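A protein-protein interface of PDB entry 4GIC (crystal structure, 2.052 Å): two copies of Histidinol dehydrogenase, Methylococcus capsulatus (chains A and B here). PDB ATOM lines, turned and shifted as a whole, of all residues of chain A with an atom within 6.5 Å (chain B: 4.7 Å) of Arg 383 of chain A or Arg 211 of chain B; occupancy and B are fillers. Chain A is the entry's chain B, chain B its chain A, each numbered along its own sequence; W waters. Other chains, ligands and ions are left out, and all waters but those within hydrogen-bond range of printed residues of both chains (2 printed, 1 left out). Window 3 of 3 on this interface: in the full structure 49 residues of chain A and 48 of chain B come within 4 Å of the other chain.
Of chain B, only Leu 130 (3.8 Å), Arg 211 (3.0 Å), Asp 213 (3.1 Å), Gln 233 (2.7 Å) and Lys 395 (3.2 Å) come within 4 Å of Arg 383 of chain A. Arg 211 of chain B touches just one residue of chain A: Arg 383 (3.0 Å). Of the printed residues of chain A, Gly 232 of chain B touches Thr 381 (3.9 Å) and Phe 384 (3.7 Å). Printed residues of chain A within 4 Å of Lys 395 of chain B: Asn 351 (2.9 Å), Ala 382 (3.2 Å), Arg 383 (3.2 Å), Phe 384 (3.9 Å) and Ser 385 (3.9 Å). Of the printed residues of chain A, Gln 233 of chain B touches Arg 383 (2.7 Å) and Phe 384 (3.9 Å). Of the printed residues of chain B, Ala 382 of chain A touches Lys 395. The nearest residue of chain A that does not touch Arg 211 of chain B is Arg 329 of chain A (6.3 Å).
No position is printed for both chains.
Among the printed residues, merely in contact across the chains: Ala 382 of chain A with Lys 395 of chain B (3.2 Å), Arg 383 of chain A with Lys 395 of chain B (3.2 Å), Phe 384 of chain A with Asp 213 of chain B (3.3 Å), Phe 384 of chain A with Gly 232 of chain B (3.7 Å), Arg 383 of chain A with Leu 130 of chain B (3.8 Å), Phe 384 of chain A with Lys 395 of chain B (3.9 Å), Thr 381 of chain A with Gly 232 of chain B (3.9 Å), Phe 384 of chain A with Gln 233 of chain B (3.9 Å), Ser 385 of chain A with Lys 395 of chain B (3.9 Å) and Phe 384 of chain A with Leu 130 of chain B (3.97 Å).
Water W2 lies within hydrogen-bond range of O of Ser 379 of chain A (2.7 Å), O of Gly 232 of chain B (2.8 Å) and NH2 of Arg 383 of chain A (2.9 Å). Water W1 lies within hydrogen-bond range of the backbone carbonyl oxygen (O) of Ala 382 of chain A (2.8 Å), the backbone NH (N) of Ala 352 of chain A (2.9 Å) and the side-chain amino group (NZ) of Lys 395 of chain B (3.1 Å).
The guanidinium group of Arg 383 of chain A lies within salt-bridge range of the side-chain carboxylate of Asp 213 of chain B. The backbone carbonyl oxygen (O) of Gln 233 of chain B is in hydrogen-bond range of the guanidinium group (NH2) of Arg 383 of chain A. The side-chain amino group of Lys 395 of chain B lies within hydrogen-bond range of the side-chain amide oxygen of Asn 351 of chain A, at 2.9 Å. The guanidinium group (NH1) of Arg 211 of chain B lies close to the guanidinium group (NH1) of Arg 383 of chain A (3.0 Å).
NE of Arg 132 of chain B is in hydrogen-bond range of O of Arg 211 of chain B (2.6 Å). The backbone carbonyl oxygen (O) of Arg 132 of chain B is in hydrogen-bond range of the backbone NH (N) of Asp 213 of chain B (2.9 Å). The side-chain carboxylate (OD1) of Asp 213 of chain B lies within salt-bridge range of the guanidinium group (NH1) of Arg 211 of chain B. The side-chain amide nitrogen (ND2) of Asn 351 of chain A lies within hydrogen-bond range of the backbone carbonyl oxygen (O) of Asn 328 of chain A (3.1 Å). The backbone carbonyl oxygen of Gly 380 of chain A lies within hydrogen-bond range of the guanidinium group of Arg 383 of chain A (3.0 Å). The side-chain hydroxyl of Ser 385 of chain A lies within hydrogen-bond range of the backbone carbonyl oxygen of Thr 381 of chain A (3.0 Å).
Of the 14 printed residues of chain B, 6 touch a printed residue of chain A. Hydrophobic or aromatic side chains of chain B that line the printed part of chain A: Leu 130. Of the 14 printed residues of chain A, 6 touch a printed residue of chain B. Hydrophobic or aromatic side chains of chain A within 4 Å of the printed part of chain B: Phe 384. Among the printed residues, 14 pairs touch across the chains. Among the printed residues, Asp or Glu carboxylates within 4 Å of a Lys or Arg side-chain nitrogen of the other chain: Arg 383 of chain A with Asp 213 of chain B.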
ATOM      1  N   ASN A 328     -18.960   4.842  13.373  1.00  0.00           N
ATOM      2  CA  ASN A 328     -17.905   4.504  12.408  1.00  0.00           C
ATOM      3  C   ASN A 328     -17.759   5.540  11.309  1.00  0.00           C
ATOM      4  O   ASN A 328     -16.670   5.713  10.757  1.00  0.00           O
ATOM      5  CB  ASN A 328     -18.100   3.104  11.824  1.00  0.00           C
ATOM      6  CG  ASN A 328     -17.680   2.024  12.796  1.00  0.00           C
ATOM      7  OD1 ASN A 328     -16.746   2.214  13.578  1.00  0.00           O
ATOM      8  ND2 ASN A 328     -18.374   0.894  12.769  1.00  0.00           N
ATOM      9  N   ARG A 329     -18.863   6.211  10.983  1.00  0.00           N
ATOM     10  CA  ARG A 329     -18.811   7.389  10.107  1.00  0.00           C
ATOM     11  C   ARG A 329     -18.180   8.609  10.787  1.00  0.00           C
ATOM     12  O   ARG A 329     -17.454   9.373  10.164  1.00  0.00           O
ATOM     13  CB  ARG A 329     -20.217   7.739   9.609  1.00  0.00           C
ATOM     14  CG  ARG A 329     -20.218   8.637   8.399  1.00  0.00           C
ATOM     15  CD  ARG A 329     -21.545   8.593   7.673  1.00  0.00           C
ATOM     16  NE  ARG A 329     -21.691   7.351   6.908  1.00  0.00           N
ATOM     17  CZ  ARG A 329     -22.260   6.228   7.349  1.00  0.00           C
ATOM     18  NH1 ARG A 329     -22.758   6.151   8.577  1.00  0.00           N
ATOM     19  NH2 ARG A 329     -22.325   5.168   6.551  1.00  0.00           N
ATOM     20  N   ILE A 330     -18.476   8.807  12.061  1.00  0.00           N
ATOM     21  CA  ILE A 330     -17.967   9.962  12.774  1.00  0.00           C
ATOM     22  C   ILE A 330     -16.470   9.806  13.026  1.00  0.00           C
ATOM     23  O   ILE A 330     -15.717  10.790  12.927  1.00  0.00           O
ATOM     24  CB  ILE A 330     -18.745  10.200  14.105  1.00  0.00           C
ATOM     25  CG1 ILE A 330     -20.193  10.597  13.807  1.00  0.00           C
ATOM     26  CG2 ILE A 330     -18.065  11.272  14.983  1.00  0.00           C
ATOM     27  CD1 ILE A 330     -21.093  10.644  15.042  1.00  0.00           C
ATOM     28  N   ALA A 331     -16.050   8.579  13.340  1.00  0.00           N
ATOM     29  CA  ALA A 331     -14.645   8.287  13.670  1.00  0.00           C
ATOM     30  C   ALA A 331     -14.135   9.257  14.747  1.00  0.00           C
ATOM     31  O   ALA A 331     -13.229  10.061  14.493  1.00  0.00           O
ATOM     32  CB  ALA A 331     -13.766   8.348  12.434  1.00  0.00           C
ATOM     33  N   ASN A 351     -13.668   2.665  13.885  1.00  0.00           N
ATOM     34  CA  ASN A 351     -12.945   3.937  13.817  1.00  0.00           C
ATOM     35  C   ASN A 351     -13.129   4.817  15.062  1.00  0.00           C
ATOM     36  O   ASN A 351     -14.162   5.474  15.213  1.00  0.00           O
ATOM     37  CB  ASN A 351     -13.388   4.703  12.565  1.00  0.00           C
ATOM     38  CG  ASN A 351     -13.178   3.898  11.290  1.00  0.00           C
ATOM     39  OD1 ASN A 351     -12.135   3.255  11.122  1.00  0.00           O
ATOM     40  ND2 ASN A 351     -14.176   3.900  10.406  1.00  0.00           N
ATOM     41  N   ALA A 352     -12.121   4.847  15.931  1.00  0.00           N
ATOM     42  CA  ALA A 352     -12.178   5.630  17.170  1.00  0.00           C
ATOM     43  C   ALA A 352     -10.773   5.687  17.765  1.00  0.00           C
ATOM     44  O   ALA A 352     -10.049   4.680  17.731  1.00  0.00           O
ATOM     45  CB  ALA A 352     -13.145   4.996  18.157  1.00  0.00           C
ATOM     46  N   PRO A 377      -6.214  10.890  17.777  1.00  0.00           N
ATOM     47  CA  PRO A 377      -6.530  11.502  16.476  1.00  0.00           C
ATOM     48  C   PRO A 377      -7.925  12.120  16.435  1.00  0.00           C
ATOM     49  O   PRO A 377      -8.899  11.447  16.788  1.00  0.00           O
ATOM     50  CB  PRO A 377      -6.453  10.310  15.491  1.00  0.00           C
ATOM     51  CG  PRO A 377      -6.752   9.085  16.347  1.00  0.00           C
ATOM     52  CD  PRO A 377      -6.216   9.411  17.735  1.00  0.00           C
ATOM     53  N   SER A 379     -10.855  15.118  14.399  1.00  0.00           N
ATOM     54  CA  SER A 379     -11.353  15.616  13.119  1.00  0.00           C
ATOM     55  C   SER A 379     -11.565  14.487  12.105  1.00  0.00           C
ATOM     56  O   SER A 379     -11.421  14.692  10.901  1.00  0.00           O
ATOM     57  CB  SER A 379     -10.405  16.671  12.545  1.00  0.00           C
ATOM     58  OG  SER A 379      -9.963  17.566  13.546  1.00  0.00           O
ATOM     59  N   GLY A 380     -11.884  13.294  12.600  1.00  0.00           N
ATOM     60  CA  GLY A 380     -12.183  12.167  11.738  1.00  0.00           C
ATOM     61  C   GLY A 380     -10.971  11.411  11.234  1.00  0.00           C
ATOM     62  O   GLY A 380     -11.120  10.476  10.436  1.00  0.00           O
ATOM     63  N   THR A 381      -9.777  11.794  11.692  1.00  0.00           N
ATOM     64  CA  THR A 381      -8.565  11.127  11.254  1.00  0.00           C
ATOM     65  C   THR A 381      -8.354   9.773  11.916  1.00  0.00           C
ATOM     66  O   THR A 381      -7.417   9.055  11.565  1.00  0.00           O
ATOM     67  CB  THR A 381      -7.300  12.003  11.450  1.00  0.00           C
ATOM     68  OG1 THR A 381      -7.031  12.174  12.849  1.00  0.00           O
ATOM     69  CG2 THR A 381      -7.508  13.361  10.763  1.00  0.00           C
ATOM     70  N   ALA A 382      -9.218   9.415  12.859  1.00  0.00           N
ATOM     71  CA  ALA A 382      -9.175   8.068  13.445  1.00  0.00           C
ATOM     72  C   ALA A 382      -9.585   7.006  12.413  1.00  0.00           C
ATOM     73  O   ALA A 382      -9.495   5.795  12.673  1.00  0.00           O
ATOM     74  CB  ALA A 382     -10.072   7.980  14.703  1.00  0.00           C
ATOM     75  N   ARG A 383     -10.052   7.453  11.249  1.00  0.00           N
ATOM     76  CA  ARG A 383     -10.270   6.541  10.121  1.00  0.00           C
ATOM     77  C   ARG A 383      -8.955   5.995   9.576  1.00  0.00           C
ATOM     78  O   ARG A 383      -8.958   4.994   8.858  1.00  0.00           O
ATOM     79  CB  ARG A 383     -11.027   7.232   8.980  1.00  0.00           C
ATOM     80  CG  ARG A 383     -12.481   7.515   9.278  1.00  0.00           C
ATOM     81  CD  ARG A 383     -13.171   8.243   8.129  1.00  0.00           C
ATOM     82  NE  ARG A 383     -12.611   9.580   7.972  1.00  0.00           N
ATOM     83  CZ  ARG A 383     -11.874   9.969   6.938  1.00  0.00           C
ATOM     84  NH1 ARG A 383     -11.644   9.139   5.920  1.00  0.00           N
ATOM     85  NH2 ARG A 383     -11.406  11.210   6.898  1.00  0.00           N
ATOM     86  N   PHE A 384      -7.843   6.670   9.856  1.00  0.00           N
ATOM     87  CA  PHE A 384      -6.553   6.229   9.288  1.00  0.00           C
ATOM     88  C   PHE A 384      -5.314   6.400  10.181  1.00  0.00           C
ATOM     89  O   PHE A 384      -4.220   6.056   9.765  1.00  0.00           O
ATOM     90  CB  PHE A 384      -6.295   6.894   7.927  1.00  0.00           C
ATOM     91  CG  PHE A 384      -6.267   8.409   7.975  1.00  0.00           C
ATOM     92  CD1 PHE A 384      -5.123   9.080   8.373  1.00  0.00           C
ATOM     93  CD2 PHE A 384      -7.380   9.151   7.599  1.00  0.00           C
ATOM     94  CE1 PHE A 384      -5.087  10.467   8.419  1.00  0.00           C
ATOM     95  CE2 PHE A 384      -7.358  10.546   7.631  1.00  0.00           C
ATOM     96  CZ  PHE A 384      -6.202  11.202   8.048  1.00  0.00           C
ATOM     97  N   SER A 385      -5.489   6.934  11.385  1.00  0.00           N
ATOM     98  CA  SER A 385      -4.372   7.218  12.294  1.00  0.00           C
ATOM     99  C   SER A 385      -4.547   6.520  13.637  1.00  0.00           C
ATOM    100  O   SER A 385      -5.687   6.215  14.058  1.00  0.00           O
ATOM    101  CB  SER A 385      -4.298   8.724  12.564  1.00  0.00           C
ATOM    102  OG  SER A 385      -4.429   9.436  11.353  1.00  0.00           O
ATOM    103  N   LEU B 130      -7.372  -0.454   7.887  1.00  0.00           N
ATOM    104  CA  LEU B 130      -8.116   0.668   7.316  1.00  0.00           C
ATOM    105  C   LEU B 130      -9.328   0.151   6.514  1.00  0.00           C
ATOM    106  O   LEU B 130      -9.235  -0.892   5.890  1.00  0.00           O
ATOM    107  CB  LEU B 130      -7.197   1.515   6.441  1.00  0.00           C
ATOM    108  CG  LEU B 130      -6.472   2.644   7.188  1.00  0.00           C
ATOM    109  CD1 LEU B 130      -5.710   2.122   8.390  1.00  0.00           C
ATOM    110  CD2 LEU B 130      -5.510   3.379   6.266  1.00  0.00           C
ATOM    111  N   ARG B 132     -10.864   1.250   3.704  1.00  0.00           N
ATOM    112  CA  ARG B 132     -10.566   1.206   2.279  1.00  0.00           C
ATOM    113  C   ARG B 132      -9.273   1.930   2.019  1.00  0.00           C
ATOM    114  O   ARG B 132      -8.955   2.914   2.686  1.00  0.00           O
ATOM    115  CB  ARG B 132     -11.671   1.859   1.444  1.00  0.00           C
ATOM    116  CG  ARG B 132     -13.055   1.233   1.608  1.00  0.00           C
ATOM    117  CD  ARG B 132     -13.975   1.638   0.465  1.00  0.00           C
ATOM    118  NE  ARG B 132     -14.679   2.876   0.739  1.00  0.00           N
ATOM    119  CZ  ARG B 132     -15.957   2.940   1.087  1.00  0.00           C
ATOM    120  NH1 ARG B 132     -16.676   1.831   1.197  1.00  0.00           N
ATOM    121  NH2 ARG B 132     -16.511   4.115   1.322  1.00  0.00           N
ATOM    122  N   LEU B 202     -10.828   9.509  -5.193  1.00  0.00           N
ATOM    123  CA  LEU B 202     -10.575   8.555  -4.104  1.00  0.00           C
ATOM    124  C   LEU B 202     -10.774   9.154  -2.711  1.00  0.00           C
ATOM    125  O   LEU B 202     -11.305   8.492  -1.809  1.00  0.00           O
ATOM    126  CB  LEU B 202      -9.149   8.005  -4.205  1.00  0.00           C
ATOM    127  CG  LEU B 202      -8.851   7.101  -5.403  1.00  0.00           C
ATOM    128  CD1 LEU B 202      -7.328   6.849  -5.487  1.00  0.00           C
ATOM    129  CD2 LEU B 202      -9.629   5.804  -5.250  1.00  0.00           C
ATOM    130  N   ALA B 203     -10.346  10.403  -2.546  1.00  0.00           N
ATOM    131  CA  ALA B 203     -10.321  11.057  -1.231  1.00  0.00           C
ATOM    132  C   ALA B 203     -11.721  11.451  -0.777  1.00  0.00           C
ATOM    133  O   ALA B 203     -12.049  11.343   0.407  1.00  0.00           O
ATOM    134  CB  ALA B 203      -9.420  12.275  -1.262  1.00  0.00           C
ATOM    135  N   TYR B 204     -12.544  11.912  -1.717  1.00  0.00           N
ATOM    136  CA  TYR B 204     -13.888  12.375  -1.382  1.00  0.00           C
ATOM    137  C   TYR B 204     -14.988  11.419  -1.854  1.00  0.00           C
ATOM    138  O   TYR B 204     -16.128  11.490  -1.400  1.00  0.00           O
ATOM    139  CB  TYR B 204     -14.112  13.773  -1.944  1.00  0.00           C
ATOM    140  CG  TYR B 204     -13.167  14.772  -1.347  1.00  0.00           C
ATOM    141  CD1 TYR B 204     -13.412  15.326  -0.087  1.00  0.00           C
ATOM    142  CD2 TYR B 204     -12.011  15.139  -2.013  1.00  0.00           C
ATOM    143  CE1 TYR B 204     -12.540  16.241   0.477  1.00  0.00           C
ATOM    144  CE2 TYR B 204     -11.125  16.048  -1.455  1.00  0.00           C
ATOM    145  CZ  TYR B 204     -11.397  16.595  -0.211  1.00  0.00           C
ATOM    146  OH  TYR B 204     -10.516  17.499   0.332  1.00  0.00           O
ATOM    147  N   GLY B 205     -14.653  10.541  -2.792  1.00  0.00           N
ATOM    148  CA  GLY B 205     -15.633   9.618  -3.332  1.00  0.00           C
ATOM    149  C   GLY B 205     -16.407  10.261  -4.462  1.00  0.00           C
ATOM    150  O   GLY B 205     -16.485  11.484  -4.543  1.00  0.00           O
ATOM    151  N   VAL B 209     -16.708   5.996  -7.758  1.00  0.00           N
ATOM    152  CA  VAL B 209     -15.496   5.683  -7.015  1.00  0.00           C
ATOM    153  C   VAL B 209     -15.697   5.781  -5.492  1.00  0.00           C
ATOM    154  O   VAL B 209     -16.079   6.830  -4.965  1.00  0.00           O
ATOM    155  CB  VAL B 209     -14.332   6.599  -7.407  1.00  0.00           C
ATOM    156  CG1 VAL B 209     -13.078   6.151  -6.675  1.00  0.00           C
ATOM    157  CG2 VAL B 209     -14.111   6.584  -8.907  1.00  0.00           C
ATOM    158  N   PRO B 210     -15.438   4.676  -4.785  1.00  0.00           N
ATOM    159  CA  PRO B 210     -15.580   4.626  -3.330  1.00  0.00           C
ATOM    160  C   PRO B 210     -14.542   5.507  -2.661  1.00  0.00           C
ATOM    161  O   PRO B 210     -13.391   5.551  -3.101  1.00  0.00           O
ATOM    162  CB  PRO B 210     -15.272   3.154  -2.998  1.00  0.00           C
ATOM    163  CG  PRO B 210     -15.451   2.405  -4.313  1.00  0.00           C
ATOM    164  CD  PRO B 210     -15.012   3.384  -5.350  1.00  0.00           C
ATOM    165  N   ARG B 211     -14.948   6.171  -1.590  1.00  0.00           N
ATOM    166  CA  ARG B 211     -14.071   7.019  -0.794  1.00  0.00           C
ATOM    167  C   ARG B 211     -13.155   6.124   0.033  1.00  0.00           C
ATOM    168  O   ARG B 211     -13.618   5.221   0.733  1.00  0.00           O
ATOM    169  CB  ARG B 211     -14.937   7.898   0.119  1.00  0.00           C
ATOM    170  CG  ARG B 211     -14.179   8.874   0.978  1.00  0.00           C
ATOM    171  CD  ARG B 211     -15.060   9.426   2.093  1.00  0.00           C
ATOM    172  NE  ARG B 211     -15.658   8.373   2.918  1.00  0.00           N
ATOM    173  CZ  ARG B 211     -15.005   7.678   3.848  1.00  0.00           C
ATOM    174  NH1 ARG B 211     -13.715   7.905   4.073  1.00  0.00           N
ATOM    175  NH2 ARG B 211     -15.637   6.743   4.546  1.00  0.00           N
ATOM    176  N   VAL B 212     -11.851   6.356  -0.047  1.00  0.00           N
ATOM    177  CA  VAL B 212     -10.913   5.538   0.703  1.00  0.00           C
ATOM    178  C   VAL B 212     -10.424   6.334   1.919  1.00  0.00           C
ATOM    179  O   VAL B 212     -10.750   7.511   2.051  1.00  0.00           O
ATOM    180  CB  VAL B 212      -9.743   5.148  -0.172  1.00  0.00           C
ATOM    181  CG1 VAL B 212     -10.285   4.461  -1.478  1.00  0.00           C
ATOM    182  CG2 VAL B 212      -8.932   6.385  -0.490  1.00  0.00           C
ATOM    183  N   ASP B 213      -9.670   5.699   2.808  1.00  0.00           N
ATOM    184  CA  ASP B 213      -9.208   6.377   4.020  1.00  0.00           C
ATOM    185  C   ASP B 213      -7.731   6.723   3.958  1.00  0.00           C
ATOM    186  O   ASP B 213      -7.199   7.457   4.806  1.00  0.00           O
ATOM    187  CB  ASP B 213      -9.538   5.514   5.225  1.00  0.00           C
ATOM    188  CG  ASP B 213     -11.022   5.182   5.281  1.00  0.00           C
ATOM    189  OD1 ASP B 213     -11.818   6.090   5.617  1.00  0.00           O
ATOM    190  OD2 ASP B 213     -11.395   4.050   4.901  1.00  0.00           O
ATOM    191  N   GLY B 232      -5.498  14.814   5.592  1.00  0.00           N
ATOM    192  CA  GLY B 232      -6.487  15.312   6.542  1.00  0.00           C
ATOM    193  C   GLY B 232      -7.822  14.651   6.220  1.00  0.00           C
ATOM    194  O   GLY B 232      -8.470  14.075   7.086  1.00  0.00           O
ATOM    195  N   GLN B 233      -8.224  14.720   4.954  1.00  0.00           N
ATOM    196  CA  GLN B 233      -9.361  13.941   4.488  1.00  0.00           C
ATOM    197  C   GLN B 233      -8.965  12.463   4.431  1.00  0.00           C
ATOM    198  O   GLN B 233      -9.762  11.580   4.755  1.00  0.00           O
ATOM    199  CB  GLN B 233      -9.814  14.442   3.113  1.00  0.00           C
ATOM    200  CG  GLN B 233     -10.938  13.651   2.475  1.00  0.00           C
ATOM    201  CD  GLN B 233     -12.226  13.661   3.285  1.00  0.00           C
ATOM    202  OE1 GLN B 233     -12.532  14.620   4.008  1.00  0.00           O
ATOM    203  NE2 GLN B 233     -13.001  12.593   3.150  1.00  0.00           N
ATOM    204  N   LYS B 395      -4.417   0.437  12.019  1.00  0.00           N
ATOM    205  CA  LYS B 395      -4.425   1.513  12.985  1.00  0.00           C
ATOM    206  C   LYS B 395      -4.791   0.935  14.352  1.00  0.00           C
ATOM    207  O   LYS B 395      -5.412  -0.152  14.441  1.00  0.00           O
ATOM    208  CB  LYS B 395      -5.365   2.640  12.559  1.00  0.00           C
ATOM    209  CG  LYS B 395      -6.807   2.207  12.360  1.00  0.00           C
ATOM    210  CD  LYS B 395      -7.629   3.343  11.794  1.00  0.00           C
ATOM    211  CE  LYS B 395      -9.000   2.882  11.311  1.00  0.00           C
ATOM    212  NZ  LYS B 395      -9.783   2.167  12.362  1.00  0.00           N
HETATM  213  O   HOH W   1      -9.622   4.033  14.788  1.00  0.00           O
HETATM  214  O   HOH W   2     -10.845  13.576   8.475  1.00  0.00           O
